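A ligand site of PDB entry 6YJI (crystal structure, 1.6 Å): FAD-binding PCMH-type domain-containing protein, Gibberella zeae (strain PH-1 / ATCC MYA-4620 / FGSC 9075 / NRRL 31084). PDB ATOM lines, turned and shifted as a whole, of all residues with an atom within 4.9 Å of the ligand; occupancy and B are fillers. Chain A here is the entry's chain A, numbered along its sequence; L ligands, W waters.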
ATOM      1  N   PHE A  36      19.792  24.446  -0.157  1.00  0.00           N
ATOM      2  CA  PHE A  36      19.525  23.419  -1.170  1.00  0.00           C
ATOM      3  C   PHE A  36      18.612  23.943  -2.264  1.00  0.00           C
ATOM      4  O   PHE A  36      18.863  23.706  -3.457  1.00  0.00           O
ATOM      5  CB  PHE A  36      18.859  22.216  -0.492  1.00  0.00           C
ATOM      6  CG  PHE A  36      18.600  21.024  -1.396  1.00  0.00           C
ATOM      7  CD1 PHE A  36      19.632  20.125  -1.692  1.00  0.00           C
ATOM      8  CD2 PHE A  36      17.333  20.774  -1.900  1.00  0.00           C
ATOM      9  CE1 PHE A  36      19.397  19.033  -2.510  1.00  0.00           C
ATOM     10  CE2 PHE A  36      17.091  19.664  -2.702  1.00  0.00           C
ATOM     11  CZ  PHE A  36      18.125  18.810  -3.023  1.00  0.00           C
ATOM     12  N   ASN A  71      15.348  32.331  13.519  1.00  0.00           N
ATOM     13  CA  ASN A  71      15.150  31.260  12.529  1.00  0.00           C
ATOM     14  C   ASN A  71      16.293  30.258  12.612  1.00  0.00           C
ATOM     15  O   ASN A  71      17.455  30.593  12.382  1.00  0.00           O
ATOM     16  CB  ASN A  71      15.036  31.879  11.120  1.00  0.00           C
ATOM     17  CG  ASN A  71      14.493  30.905  10.072  1.00  0.00           C
ATOM     18  OD1 ASN A  71      13.309  30.940   9.720  1.00  0.00           O
ATOM     19  ND2 ASN A  71      15.372  30.015   9.583  1.00  0.00           N
ATOM     20  N   ALA A  72      15.953  29.017  12.976  1.00  0.00           N
ATOM     21  CA  ALA A  72      16.965  27.981  13.126  1.00  0.00           C
ATOM     22  C   ALA A  72      17.421  27.513  11.750  1.00  0.00           C
ATOM     23  O   ALA A  72      16.592  27.241  10.889  1.00  0.00           O
ATOM     24  CB  ALA A  72      16.406  26.807  13.948  1.00  0.00           C
ATOM     25  N   LEU A  73      18.731  27.438  11.559  1.00  0.00           N
ATOM     26  CA  LEU A  73      19.320  26.878  10.338  1.00  0.00           C
ATOM     27  C   LEU A  73      19.937  25.528  10.666  1.00  0.00           C
ATOM     28  O   LEU A  73      20.919  25.456  11.418  1.00  0.00           O
ATOM     29  CB  LEU A  73      20.385  27.815   9.758  1.00  0.00           C
ATOM     30  CG  LEU A  73      21.197  27.246   8.602  1.00  0.00           C
ATOM     31  CD1 LEU A  73      20.283  26.831   7.479  1.00  0.00           C
ATOM     32  CD2 LEU A  73      22.201  28.327   8.189  1.00  0.00           C
ATOM     33  N   GLY A  74      19.362  24.467  10.089  1.00  0.00           N
ATOM     34  CA  GLY A  74      19.942  23.134  10.152  1.00  0.00           C
ATOM     35  C   GLY A  74      20.791  22.898   8.911  1.00  0.00           C
ATOM     36  O   GLY A  74      21.426  23.811   8.409  1.00  0.00           O
ATOM     37  N   PRO A  75      20.822  21.670   8.387  1.00  0.00           N
ATOM     38  CA  PRO A  75      21.635  21.398   7.185  1.00  0.00           C
ATOM     39  C   PRO A  75      21.168  22.053   5.886  1.00  0.00           C
ATOM     40  O   PRO A  75      21.829  21.858   4.861  1.00  0.00           O
ATOM     41  CB  PRO A  75      21.563  19.857   7.079  1.00  0.00           C
ATOM     42  CG  PRO A  75      21.477  19.442   8.532  1.00  0.00           C
ATOM     43  CD  PRO A  75      20.437  20.402   9.062  1.00  0.00           C
ATOM     44  N   ALA A  76      20.075  22.841   5.902  1.00  0.00           N
ATOM     45  CA  ALA A  76      19.677  23.732   4.800  1.00  0.00           C
ATOM     46  C   ALA A  76      18.930  23.017   3.682  1.00  0.00           C
ATOM     47  O   ALA A  76      18.998  23.433   2.513  1.00  0.00           O
ATOM     48  CB  ALA A  76      20.903  24.450   4.219  1.00  0.00           C
ATOM     49  N   HIS A  77      18.225  21.907   4.006  1.00  0.00           N
ATOM     50  CA  HIS A  77      17.532  21.153   2.961  1.00  0.00           C
ATOM     51  C   HIS A  77      16.135  21.660   2.593  1.00  0.00           C
ATOM     52  O   HIS A  77      15.595  21.185   1.583  1.00  0.00           O
ATOM     53  CB  HIS A  77      17.460  19.659   3.349  1.00  0.00           C
ATOM     54  CG  HIS A  77      18.677  18.897   2.917  1.00  0.00           C
ATOM     55  ND1 HIS A  77      18.741  18.248   1.696  1.00  0.00           N
ATOM     56  CD2 HIS A  77      19.918  18.829   3.447  1.00  0.00           C
ATOM     57  CE1 HIS A  77      19.941  17.717   1.556  1.00  0.00           C
ATOM     58  NE2 HIS A  77      20.686  18.087   2.586  1.00  0.00           N
ATOM     59  N   SER A  78      15.559  22.651   3.292  1.00  0.00           N
ATOM     60  CA  SER A  78      14.145  23.001   3.070  1.00  0.00           C
ATOM     61  C   SER A  78      13.841  23.287   1.585  1.00  0.00           C
ATOM     62  O   SER A  78      14.504  24.121   0.933  1.00  0.00           O
ATOM     63  CB  SER A  78      13.754  24.237   3.904  1.00  0.00           C
ATOM     64  OG  SER A  78      12.411  24.641   3.673  1.00  0.00           O
ATOM     65  N   PHE A  79      12.829  22.574   1.068  1.00  0.00           N
ATOM     66  CA  PHE A  79      12.387  22.846  -0.292  1.00  0.00           C
ATOM     67  C   PHE A  79      11.685  24.185  -0.395  1.00  0.00           C
ATOM     68  O   PHE A  79      11.463  24.695  -1.507  1.00  0.00           O
ATOM     69  CB  PHE A  79      11.431  21.769  -0.799  1.00  0.00           C
ATOM     70  CG  PHE A  79      12.006  20.358  -0.860  1.00  0.00           C
ATOM     71  CD1 PHE A  79      13.359  20.065  -0.686  1.00  0.00           C
ATOM     72  CD2 PHE A  79      11.131  19.303  -1.108  1.00  0.00           C
ATOM     73  CE1 PHE A  79      13.812  18.690  -0.733  1.00  0.00           C
ATOM     74  CE2 PHE A  79      11.580  17.953  -1.174  1.00  0.00           C
ATOM     75  CZ  PHE A  79      12.921  17.673  -1.017  1.00  0.00           C
ATOM     76  N   ASN A  82      13.228  27.357   4.192  1.00  0.00           N
ATOM     77  CA  ASN A  82      12.930  27.707   5.576  1.00  0.00           C
ATOM     78  C   ASN A  82      14.149  27.724   6.479  1.00  0.00           C
ATOM     79  O   ASN A  82      14.075  28.308   7.582  1.00  0.00           O
ATOM     80  CB  ASN A  82      11.908  26.748   6.190  1.00  0.00           C
ATOM     81  CG  ASN A  82      10.548  26.795   5.512  1.00  0.00           C
ATOM     82  OD1 ASN A  82      10.224  27.719   4.738  1.00  0.00           O
ATOM     83  ND2 ASN A  82       9.717  25.803   5.812  1.00  0.00           N
ATOM     84  N   GLY A  83      15.284  27.151   6.047  1.00  0.00           N
ATOM     85  CA  GLY A  83      16.506  27.241   6.820  1.00  0.00           C
ATOM     86  C   GLY A  83      16.919  28.670   7.094  1.00  0.00           C
ATOM     87  O   GLY A  83      17.550  28.954   8.127  1.00  0.00           O
ATOM     88  N   MET A  94      22.744  25.934  13.620  1.00  0.00           N
ATOM     89  CA  MET A  94      22.732  24.949  14.709  1.00  0.00           C
ATOM     90  C   MET A  94      23.815  23.866  14.566  1.00  0.00           C
ATOM     91  O   MET A  94      23.757  22.829  15.261  1.00  0.00           O
ATOM     92  CB  MET A  94      21.340  24.300  14.787  1.00  0.00           C
ATOM     93  CG  MET A  94      20.205  25.257  15.209  1.00  0.00           C
ATOM     94  SD  MET A  94      20.473  25.952  16.832  1.00  0.00           S
ATOM     95  CE  MET A  94      20.206  24.495  17.882  1.00  0.00           C
ATOM     96  N   GLY A 113      20.138  19.274  17.921  1.00  0.00           N
ATOM     97  CA  GLY A 113      19.326  20.081  17.023  1.00  0.00           C
ATOM     98  C   GLY A 113      19.954  20.378  15.672  1.00  0.00           C
ATOM     99  O   GLY A 113      19.250  20.867  14.789  1.00  0.00           O
ATOM    100  N   GLY A 114      21.244  20.102  15.503  1.00  0.00           N
ATOM    101  CA  GLY A 114      21.894  20.276  14.217  1.00  0.00           C
ATOM    102  C   GLY A 114      22.445  18.990  13.613  1.00  0.00           C
ATOM    103  O   GLY A 114      23.294  19.080  12.711  1.00  0.00           O
ATOM    104  N   VAL A 135      14.401   9.994   6.426  1.00  0.00           N
ATOM    105  CA  VAL A 135      14.286  10.468   5.032  1.00  0.00           C
ATOM    106  C   VAL A 135      15.427   9.900   4.186  1.00  0.00           C
ATOM    107  O   VAL A 135      16.440   9.381   4.665  1.00  0.00           O
ATOM    108  CB  VAL A 135      14.276  11.999   5.003  1.00  0.00           C
ATOM    109  CG1 VAL A 135      13.080  12.509   5.808  1.00  0.00           C
ATOM    110  CG2 VAL A 135      15.587  12.611   5.531  1.00  0.00           C
ATOM    111  N   ARG A 136      15.250  10.025   2.846  1.00  0.00           N
ATOM    112  CA  ARG A 136      16.138   9.384   1.872  1.00  0.00           C
ATOM    113  C   ARG A 136      17.262  10.330   1.468  1.00  0.00           C
ATOM    114  O   ARG A 136      17.468  10.676   0.298  1.00  0.00           O
ATOM    115  CB  ARG A 136      15.354   8.922   0.634  1.00  0.00           C
ATOM    116  CG  ARG A 136      14.100   8.116   0.985  1.00  0.00           C
ATOM    117  CD  ARG A 136      13.431   7.442  -0.211  1.00  0.00           C
ATOM    118  NE  ARG A 136      12.096   7.007   0.166  1.00  0.00           N
ATOM    119  CZ  ARG A 136      11.346   6.115  -0.480  1.00  0.00           C
ATOM    120  NH1 ARG A 136      11.817   5.487  -1.557  1.00  0.00           N
ATOM    121  NH2 ARG A 136      10.146   5.784  -0.002  1.00  0.00           N
ATOM    122  N   GLY A 137      17.992  10.778   2.481  1.00  0.00           N
ATOM    123  CA  GLY A 137      19.085  11.704   2.312  1.00  0.00           C
ATOM    124  C   GLY A 137      19.884  11.796   3.590  1.00  0.00           C
ATOM    125  O   GLY A 137      19.409  12.321   4.595  1.00  0.00           O
ATOM    126  N   VAL A 140      20.474  15.240   5.367  1.00  0.00           N
ATOM    127  CA  VAL A 140      19.351  16.026   5.847  1.00  0.00           C
ATOM    128  C   VAL A 140      19.369  16.106   7.363  1.00  0.00           C
ATOM    129  O   VAL A 140      19.760  15.173   8.075  1.00  0.00           O
ATOM    130  CB  VAL A 140      18.044  15.401   5.314  1.00  0.00           C
ATOM    131  CG1 VAL A 140      16.818  16.191   5.799  1.00  0.00           C
ATOM    132  CG2 VAL A 140      18.030  15.357   3.776  1.00  0.00           C
ATOM    133  N   GLY A 141      18.924  17.261   7.877  1.00  0.00           N
ATOM    134  CA  GLY A 141      18.733  17.434   9.312  1.00  0.00           C
ATOM    135  C   GLY A 141      17.749  16.444   9.909  1.00  0.00           C
ATOM    136  O   GLY A 141      16.627  16.331   9.412  1.00  0.00           O
ATOM    137  N   THR A 143      16.417  16.791  12.874  1.00  0.00           N
ATOM    138  CA  THR A 143      15.400  17.597  13.563  1.00  0.00           C
ATOM    139  C   THR A 143      14.420  18.209  12.570  1.00  0.00           C
ATOM    140  O   THR A 143      13.197  18.001  12.675  1.00  0.00           O
ATOM    141  CB  THR A 143      16.082  18.646  14.414  1.00  0.00           C
ATOM    142  OG1 THR A 143      17.033  18.016  15.282  1.00  0.00           O
ATOM    143  CG2 THR A 143      15.052  19.413  15.273  1.00  0.00           C
ATOM    144  N   GLY A 144      14.934  18.927  11.584  1.00  0.00           N
ATOM    145  CA  GLY A 144      14.057  19.535  10.585  1.00  0.00           C
ATOM    146  C   GLY A 144      13.176  18.504   9.893  1.00  0.00           C
ATOM    147  O   GLY A 144      11.979  18.734   9.729  1.00  0.00           O
ATOM    148  N   SER A 145      13.760  17.391   9.480  1.00  0.00           N
ATOM    149  CA  SER A 145      12.944  16.396   8.764  1.00  0.00           C
ATOM    150  C   SER A 145      11.893  15.765   9.679  1.00  0.00           C
ATOM    151  O   SER A 145      10.782  15.485   9.249  1.00  0.00           O
ATOM    152  CB  SER A 145      13.812  15.319   8.122  1.00  0.00           C
ATOM    153  OG  SER A 145      14.535  14.541   9.030  1.00  0.00           O
ATOM    154  N   ILE A 147      10.257  17.103  12.317  1.00  0.00           N
ATOM    155  CA  ILE A 147       9.141  17.983  12.693  1.00  0.00           C
ATOM    156  C   ILE A 147       8.205  18.252  11.532  1.00  0.00           C
ATOM    157  O   ILE A 147       7.153  18.894  11.719  1.00  0.00           O
ATOM    158  CB  ILE A 147       9.623  19.322  13.314  1.00  0.00           C
ATOM    159  CG1 ILE A 147      10.479  20.117  12.329  1.00  0.00           C
ATOM    160  CG2 ILE A 147      10.428  19.001  14.612  1.00  0.00           C
ATOM    161  CD1 ILE A 147      10.906  21.504  12.841  1.00  0.00           C
ATOM    162  N   GLY A 150       8.556  13.147   7.554  1.00  0.00           N
ATOM    163  CA  GLY A 150       9.782  12.428   7.299  1.00  0.00           C
ATOM    164  C   GLY A 150       9.660  11.010   6.775  1.00  0.00           C
ATOM    165  O   GLY A 150      10.677  10.292   6.757  1.00  0.00           O
ATOM    166  N   PHE A 151       8.473  10.606   6.343  1.00  0.00           N
ATOM    167  CA  PHE A 151       8.190   9.263   5.846  1.00  0.00           C
ATOM    168  C   PHE A 151       9.342   8.666   5.064  1.00  0.00           C
ATOM    169  O   PHE A 151       9.798   9.230   4.068  1.00  0.00           O
ATOM    170  CB  PHE A 151       6.924   9.311   4.968  1.00  0.00           C
ATOM    171  CG  PHE A 151       6.449   7.953   4.471  1.00  0.00           C
ATOM    172  CD1 PHE A 151       6.945   7.432   3.288  1.00  0.00           C
ATOM    173  CD2 PHE A 151       5.515   7.230   5.157  1.00  0.00           C
ATOM    174  CE1 PHE A 151       6.550   6.212   2.831  1.00  0.00           C
ATOM    175  CE2 PHE A 151       5.091   6.003   4.698  1.00  0.00           C
ATOM    176  CZ  PHE A 151       5.606   5.493   3.503  1.00  0.00           C
ATOM    177  N   ALA A 195       9.083  24.464  14.228  1.00  0.00           N
ATOM    178  CA  ALA A 195       9.842  25.712  14.173  1.00  0.00           C
ATOM    179  C   ALA A 195       9.086  26.902  14.771  1.00  0.00           C
ATOM    180  O   ALA A 195       9.710  27.911  15.085  1.00  0.00           O
ATOM    181  CB  ALA A 195      10.220  26.103  12.736  1.00  0.00           C
ATOM    182  N   GLY A 198       9.965  27.322  19.137  1.00  0.00           N
ATOM    183  CA  GLY A 198      11.239  27.535  19.803  1.00  0.00           C
ATOM    184  C   GLY A 198      12.402  26.940  19.021  1.00  0.00           C
ATOM    185  O   GLY A 198      12.250  26.456  17.897  1.00  0.00           O
ATOM    186  N   ILE A 199      13.573  26.977  19.645  1.00  0.00           N
ATOM    187  CA  ILE A 199      14.772  26.333  19.097  1.00  0.00           C
ATOM    188  C   ILE A 199      14.911  24.966  19.759  1.00  0.00           C
ATOM    189  O   ILE A 199      14.966  24.865  20.989  1.00  0.00           O
ATOM    190  CB  ILE A 199      16.018  27.192  19.322  1.00  0.00           C
ATOM    191  CG1 ILE A 199      15.823  28.606  18.733  1.00  0.00           C
ATOM    192  CG2 ILE A 199      17.234  26.540  18.683  1.00  0.00           C
ATOM    193  CD1 ILE A 199      15.677  28.647  17.202  1.00  0.00           C
ATOM    194  N   ILE A 200      14.982  23.924  18.945  1.00  0.00           N
ATOM    195  CA  ILE A 200      15.142  22.556  19.440  1.00  0.00           C
ATOM    196  C   ILE A 200      16.620  22.290  19.654  1.00  0.00           C
ATOM    197  O   ILE A 200      17.417  22.352  18.701  1.00  0.00           O
ATOM    198  CB  ILE A 200      14.501  21.539  18.478  1.00  0.00           C
ATOM    199  CG1 ILE A 200      13.000  21.873  18.377  1.00  0.00           C
ATOM    200  CG2 ILE A 200      14.851  20.102  18.948  1.00  0.00           C
ATOM    201  CD1 ILE A 200      12.226  21.069  17.327  1.00  0.00           C
ATOM    202  N   PHE A 431       1.583  17.611   2.892  1.00  0.00           N
ATOM    203  CA  PHE A 431       2.705  16.950   3.581  1.00  0.00           C
ATOM    204  C   PHE A 431       3.698  18.048   3.916  1.00  0.00           C
ATOM    205  O   PHE A 431       4.196  18.719   3.018  1.00  0.00           O
ATOM    206  CB  PHE A 431       3.316  15.860   2.676  1.00  0.00           C
ATOM    207  CG  PHE A 431       4.425  15.089   3.304  1.00  0.00           C
ATOM    208  CD1 PHE A 431       4.204  14.273   4.372  1.00  0.00           C
ATOM    209  CD2 PHE A 431       5.719  15.180   2.802  1.00  0.00           C
ATOM    210  CE1 PHE A 431       5.253  13.553   4.965  1.00  0.00           C
ATOM    211  CE2 PHE A 431       6.751  14.456   3.362  1.00  0.00           C
ATOM    212  CZ  PHE A 431       6.498  13.639   4.447  1.00  0.00           C
ATOM    213  N   ASN A 433       6.877  18.444   4.949  1.00  0.00           N
ATOM    214  CA  ASN A 433       8.193  18.522   4.305  1.00  0.00           C
ATOM    215  C   ASN A 433       8.087  18.844   2.815  1.00  0.00           C
ATOM    216  O   ASN A 433       9.034  19.383   2.213  1.00  0.00           O
ATOM    217  CB  ASN A 433       8.969  17.193   4.489  1.00  0.00           C
ATOM    218  CG  ASN A 433       9.537  17.049   5.866  1.00  0.00           C
ATOM    219  OD1 ASN A 433       9.608  18.018   6.607  1.00  0.00           O
ATOM    220  ND2 ASN A 433       9.922  15.812   6.243  1.00  0.00           N
ATOM    221  N   TYR A 434       6.967  18.516   2.198  1.00  0.00           N
ATOM    222  CA  TYR A 434       6.718  18.900   0.805  1.00  0.00           C
ATOM    223  C   TYR A 434       5.709  20.050   0.702  1.00  0.00           C
ATOM    224  O   TYR A 434       4.790  20.047  -0.143  1.00  0.00           O
ATOM    225  CB  TYR A 434       6.239  17.710  -0.035  1.00  0.00           C
ATOM    226  CG  TYR A 434       7.183  16.497  -0.132  1.00  0.00           C
ATOM    227  CD1 TYR A 434       8.494  16.580   0.241  1.00  0.00           C
ATOM    228  CD2 TYR A 434       6.716  15.302  -0.661  1.00  0.00           C
ATOM    229  CE1 TYR A 434       9.352  15.430   0.154  1.00  0.00           C
ATOM    230  CE2 TYR A 434       7.541  14.164  -0.757  1.00  0.00           C
ATOM    231  CZ  TYR A 434       8.841  14.248  -0.375  1.00  0.00           C
ATOM    232  OH  TYR A 434       9.606  13.116  -0.513  1.00  0.00           O
ATOM    233  N   HIS A 472       8.671  31.982   8.725  1.00  0.00           N
ATOM    234  CA  HIS A 472       8.521  31.623   7.316  1.00  0.00           C
ATOM    235  C   HIS A 472       7.047  31.741   6.896  1.00  0.00           C
ATOM    236  O   HIS A 472       6.163  32.033   7.710  1.00  0.00           O
ATOM    237  CB  HIS A 472       9.119  30.220   7.021  1.00  0.00           C
ATOM    238  CG  HIS A 472       8.366  29.065   7.609  1.00  0.00           C
ATOM    239  ND1 HIS A 472       8.561  28.627   8.906  1.00  0.00           N
ATOM    240  CD2 HIS A 472       7.479  28.210   7.049  1.00  0.00           C
ATOM    241  CE1 HIS A 472       7.787  27.585   9.124  1.00  0.00           C
ATOM    242  NE2 HIS A 472       7.130  27.303   8.023  1.00  0.00           N
HETATM  243  P1  LIG L   1      16.680  23.450   7.077  1.00  0.00           P
HETATM  244  O1  LIG L   1      16.324  24.116   5.779  1.00  0.00           O
HETATM  245  O2  LIG L   1      17.987  23.914   7.675  1.00  0.00           O
HETATM  246  O3  LIG L   1      15.579  23.538   8.131  1.00  0.00           O
HETATM  247  C1  LIG L   1      14.222  23.120   7.841  1.00  0.00           C
HETATM  248  C2  LIG L   1      13.212  23.718   8.791  1.00  0.00           C
HETATM  249  O4  LIG L   1      13.327  23.081  10.089  1.00  0.00           O
HETATM  250  C3  LIG L   1      13.299  25.232   9.056  1.00  0.00           C
HETATM  251  O5  LIG L   1      11.996  25.727   9.332  1.00  0.00           O
HETATM  252  C4  LIG L   1      14.140  25.277  10.334  1.00  0.00           C
HETATM  253  O6  LIG L   1      13.975  26.495  11.056  1.00  0.00           O
HETATM  254  C5  LIG L   1      13.609  24.040  11.085  1.00  0.00           C
HETATM  255  N1  LIG L   1      14.596  23.507  12.022  1.00  0.00           N
HETATM  256  C6  LIG L   1      15.733  22.785  11.745  1.00  0.00           C
HETATM  257  N2  LIG L   1      16.456  22.491  12.801  1.00  0.00           N
HETATM  258  C7  LIG L   1      15.766  23.097  13.845  1.00  0.00           C
HETATM  259  C8  LIG L   1      16.030  23.170  15.237  1.00  0.00           C
HETATM  260  N3  LIG L   1      17.084  22.616  15.839  1.00  0.00           N
HETATM  261  N4  LIG L   1      15.119  23.792  15.991  1.00  0.00           N
HETATM  262  C9  LIG L   1      14.052  24.353  15.416  1.00  0.00           C
HETATM  263  N5  LIG L   1      13.696  24.344  14.129  1.00  0.00           N
HETATM  264  C10 LIG L   1      14.609  23.706  13.391  1.00  0.00           C
HETATM  265  N6  LIG L   1      11.598  14.913   3.273  1.00  0.00           N
HETATM  266  C11 LIG L   1      10.856  13.781   3.462  1.00  0.00           C
HETATM  267  O7  LIG L   1       9.779  13.793   4.076  1.00  0.00           O
HETATM  268  N7  LIG L   1      11.280  12.592   2.925  1.00  0.00           N
HETATM  269  C12 LIG L   1      12.456  12.380   2.241  1.00  0.00           C
HETATM  270  O8  LIG L   1      12.756  11.235   1.895  1.00  0.00           O
HETATM  271  C13 LIG L   1      13.268  13.560   2.089  1.00  0.00           C
HETATM  272  N8  LIG L   1      14.413  13.427   1.460  1.00  0.00           N
HETATM  273  C14 LIG L   1      15.171  14.582   1.266  1.00  0.00           C
HETATM  274  C15 LIG L   1      16.399  14.456   0.614  1.00  0.00           C
HETATM  275  C16 LIG L   1      17.204  15.586   0.413  1.00  0.00           C
HETATM  276  C17 LIG L   1      18.514  15.428  -0.312  1.00  0.00           C
HETATM  277  C18 LIG L   1      16.781  16.838   0.887  1.00  0.00           C
HETATM  278  C19 LIG L   1      17.645  18.059   0.728  1.00  0.00           C
HETATM  279  C20 LIG L   1      15.575  16.947   1.569  1.00  0.00           C
HETATM  280  C21 LIG L   1      14.758  15.837   1.740  1.00  0.00           C
HETATM  281  N9  LIG L   1      13.528  15.918   2.417  1.00  0.00           N
HETATM  282  C22 LIG L   1      12.752  14.800   2.607  1.00  0.00           C
HETATM  283  C23 LIG L   1      13.031  17.220   2.918  1.00  0.00           C
HETATM  284  C24 LIG L   1      13.504  17.560   4.314  1.00  0.00           C
HETATM  285  O9  LIG L   1      13.053  16.530   5.209  1.00  0.00           O
HETATM  286  C25 LIG L   1      12.901  18.906   4.721  1.00  0.00           C
HETATM  287  O10 LIG L   1      13.300  19.865   3.747  1.00  0.00           O
HETATM  288  C26 LIG L   1      13.405  19.398   6.071  1.00  0.00           C
HETATM  289  O11 LIG L   1      12.702  20.596   6.451  1.00  0.00           O
HETATM  290  C27 LIG L   1      14.899  19.653   6.041  1.00  0.00           C
HETATM  291  O12 LIG L   1      15.350  19.974   7.366  1.00  0.00           O
HETATM  292  P2  LIG L   1      16.826  20.466   7.616  1.00  0.00           P
HETATM  293  O13 LIG L   1      17.000  20.788   9.094  1.00  0.00           O
HETATM  294  O14 LIG L   1      17.792  19.610   6.936  1.00  0.00           O
HETATM  295  O15 LIG L   1      16.790  21.878   6.815  1.00  0.00           O
HETATM  296  O   HOH W   1       8.740  11.230   2.988  1.00  0.00           O
HETATM  297  O   HOH W   2      12.318  10.782  -0.775  1.00  0.00           O
HETATM  298  O   HOH W   3      17.807  20.184  11.623  1.00  0.00           O
HETATM  299  O   HOH W   4      13.265  28.154  13.034  1.00  0.00           O
HETATM  300  O   HOH W   5      11.298  22.889   5.471  1.00  0.00           O
HETATM  301  O   HOH W   6      11.704  28.459   9.526  1.00  0.00           O
HETATM  302  O   HOH W   7      16.702  26.132   3.996  1.00  0.00           O
HETATM  303  O   HOH W   8       9.392  24.768   9.529  1.00  0.00           O
HETATM  304  O   HOH W   9      11.089  20.988   2.822  1.00  0.00           O
HETATM  305  O   HOH W  10      10.534  20.337   8.196  1.00  0.00           O
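The backbone NH of His 77 is in hydrogen-bond range of an oxygen (O15) of the ligand (3.2 Å).
An oxygen (O10) of the ligand lies within hydrogen-bond range of the backbone carbonyl oxygen (O) of His 77, at 3.4 Å.
ND1 of His 77 is bonded to C19 of the ligand (1.5 Å).
O6 of the ligand lies within hydrogen-bond range of O of Ala 72 (2.7 Å).
N of Gly 141 sits at hydrogen-bond distance from O14 of the ligand (2.8 Å).
N of Gly 74 is in hydrogen-bond range of O2 of the ligand.
N4 of the ligand lies within hydrogen-bond range of N of Ile 200, at 3.0 Å.
The backbone carbonyl oxygen of Ile 200 sits at hydrogen-bond distance from a nitrogen (N3) of the ligand (2.9 Å).
O8 of the ligand is in hydrogen-bond range of N of Arg 136, 2.9 Å away.
O2 of the ligand sits at hydrogen-bond distance from N of Ala 76, 2.9 Å away.
The side-chain amide nitrogen (ND2) of Asn 433 is in hydrogen-bond range of an oxygen (O7) of the ligand (3.0 Å).
N3 of the ligand sits at hydrogen-bond distance from O of Gly 113 (3.0 Å).
The backbone NH (N) of Ser 78 is in hydrogen-bond range of an oxygen (O1) of the ligand (3.0 Å).
The backbone NH (N) of Gly 83 is in hydrogen-bond range of an oxygen (O1) of the ligand, at 3.2 Å.
The backbone carbonyl oxygen (O) of Gly 141 lies within hydrogen-bond range of the side-chain hydroxyl (OG) of Ser 145 (2.8 Å).
The backbone carbonyl oxygen (O) of Ala 76 lies within hydrogen-bond range of the backbone NH (N) of Phe 36 (3.0 Å).
ND2 of Asn 433 lies within hydrogen-bond range of O of Ser 145 (3.1 Å).
The side-chain amide nitrogen (ND2) of Asn 433 lies close to the backbone NH (N) of Gly 150 (3.3 Å).
N of Asn 82 lies within hydrogen-bond range of OG of Ser 78 (2.9 Å).
O of Gly 83 is in hydrogen-bond range of ND2 of Asn 71 (2.8 Å).
The backbone carbonyl oxygen (O) of Asn 82 is in hydrogen-bond range of the side-chain amide nitrogen (ND2) of Asn 71 (2.9 Å).
The backbone carbonyl oxygen of Leu 73 is in hydrogen-bond range of the backbone NH of Met 94 (2.9 Å).
CD1 of Phe 36 touches C19 of the ligand, 3.8 Å away.
Leu 73 touches the ligand (CD1 to O2, 3.7 Å).
Pro 75 touches the ligand (CD to O13, 3.5 Å).
CE1 of Phe 79 touches C20 of the ligand, 3.4 Å away.
Asn 82 touches the ligand.
CB of Val 135 touches C12 of the ligand, at 3.3 Å.
CG2 of Val 140 touches C16 of the ligand, 3.5 Å away.
CG2 of Thr 143 touches N3 of the ligand (3.8 Å).
Gly 144 touches the ligand.
Ser 145 touches the ligand (CB to O9, 3.2 Å).
CD1 of Ile 147 touches O4 of the ligand, at 3.99 Å.
Gly 150 touches the ligand.
O of Phe 151 touches N7 of the ligand, 3.8 Å away.
Ala 195 touches the ligand.
O of Gly 198 touches C9 of the ligand, 3.7 Å away.
Ile 199 touches the ligand (C to N4, 3.95 Å).
CE2 of Phe 431 touches O7 of the ligand, at 3.2 Å.
Tyr 434 touches the ligand.
Hydrophobic or aromatic side chains within 4 Å of the ligand: Phe 36, Ala 72, Leu 73, Pro 75, His 77, Phe 79, Val 135, Val 140, Ile 147, Ala 195, Ile 200, Phe 431 and Tyr 434.
Of the 34 residues printed, 29 come within 4 Å of the ligand.
The nearest printed residue that does not touch the ligand is Asn 71 (4.1 Å).
Water W9 lies within hydrogen-bond range of O10 of the ligand, O of Asn 433 and N of Phe 79.
Water W4 bridges O6 of the ligand (2.7 Å) and N of Ala 72 (2.8 Å).
Water W7 lies within hydrogen-bond range of N of Gly 83 and O1 of the ligand.
Water W3 lies within hydrogen-bond range of an oxygen (O13) of the ligand (2.7 Å) and the backbone NH of Gly 144 (3.1 Å).
Water W10 lies within hydrogen-bond range of O of Gly 144 (2.6 Å), O11 of the ligand (2.8 Å) and OD1 of Asn 433 (3.0 Å).
Water W1 lies within hydrogen-bond range of O of Phe 151 (2.5 Å) and N7 of the ligand (2.9 Å).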
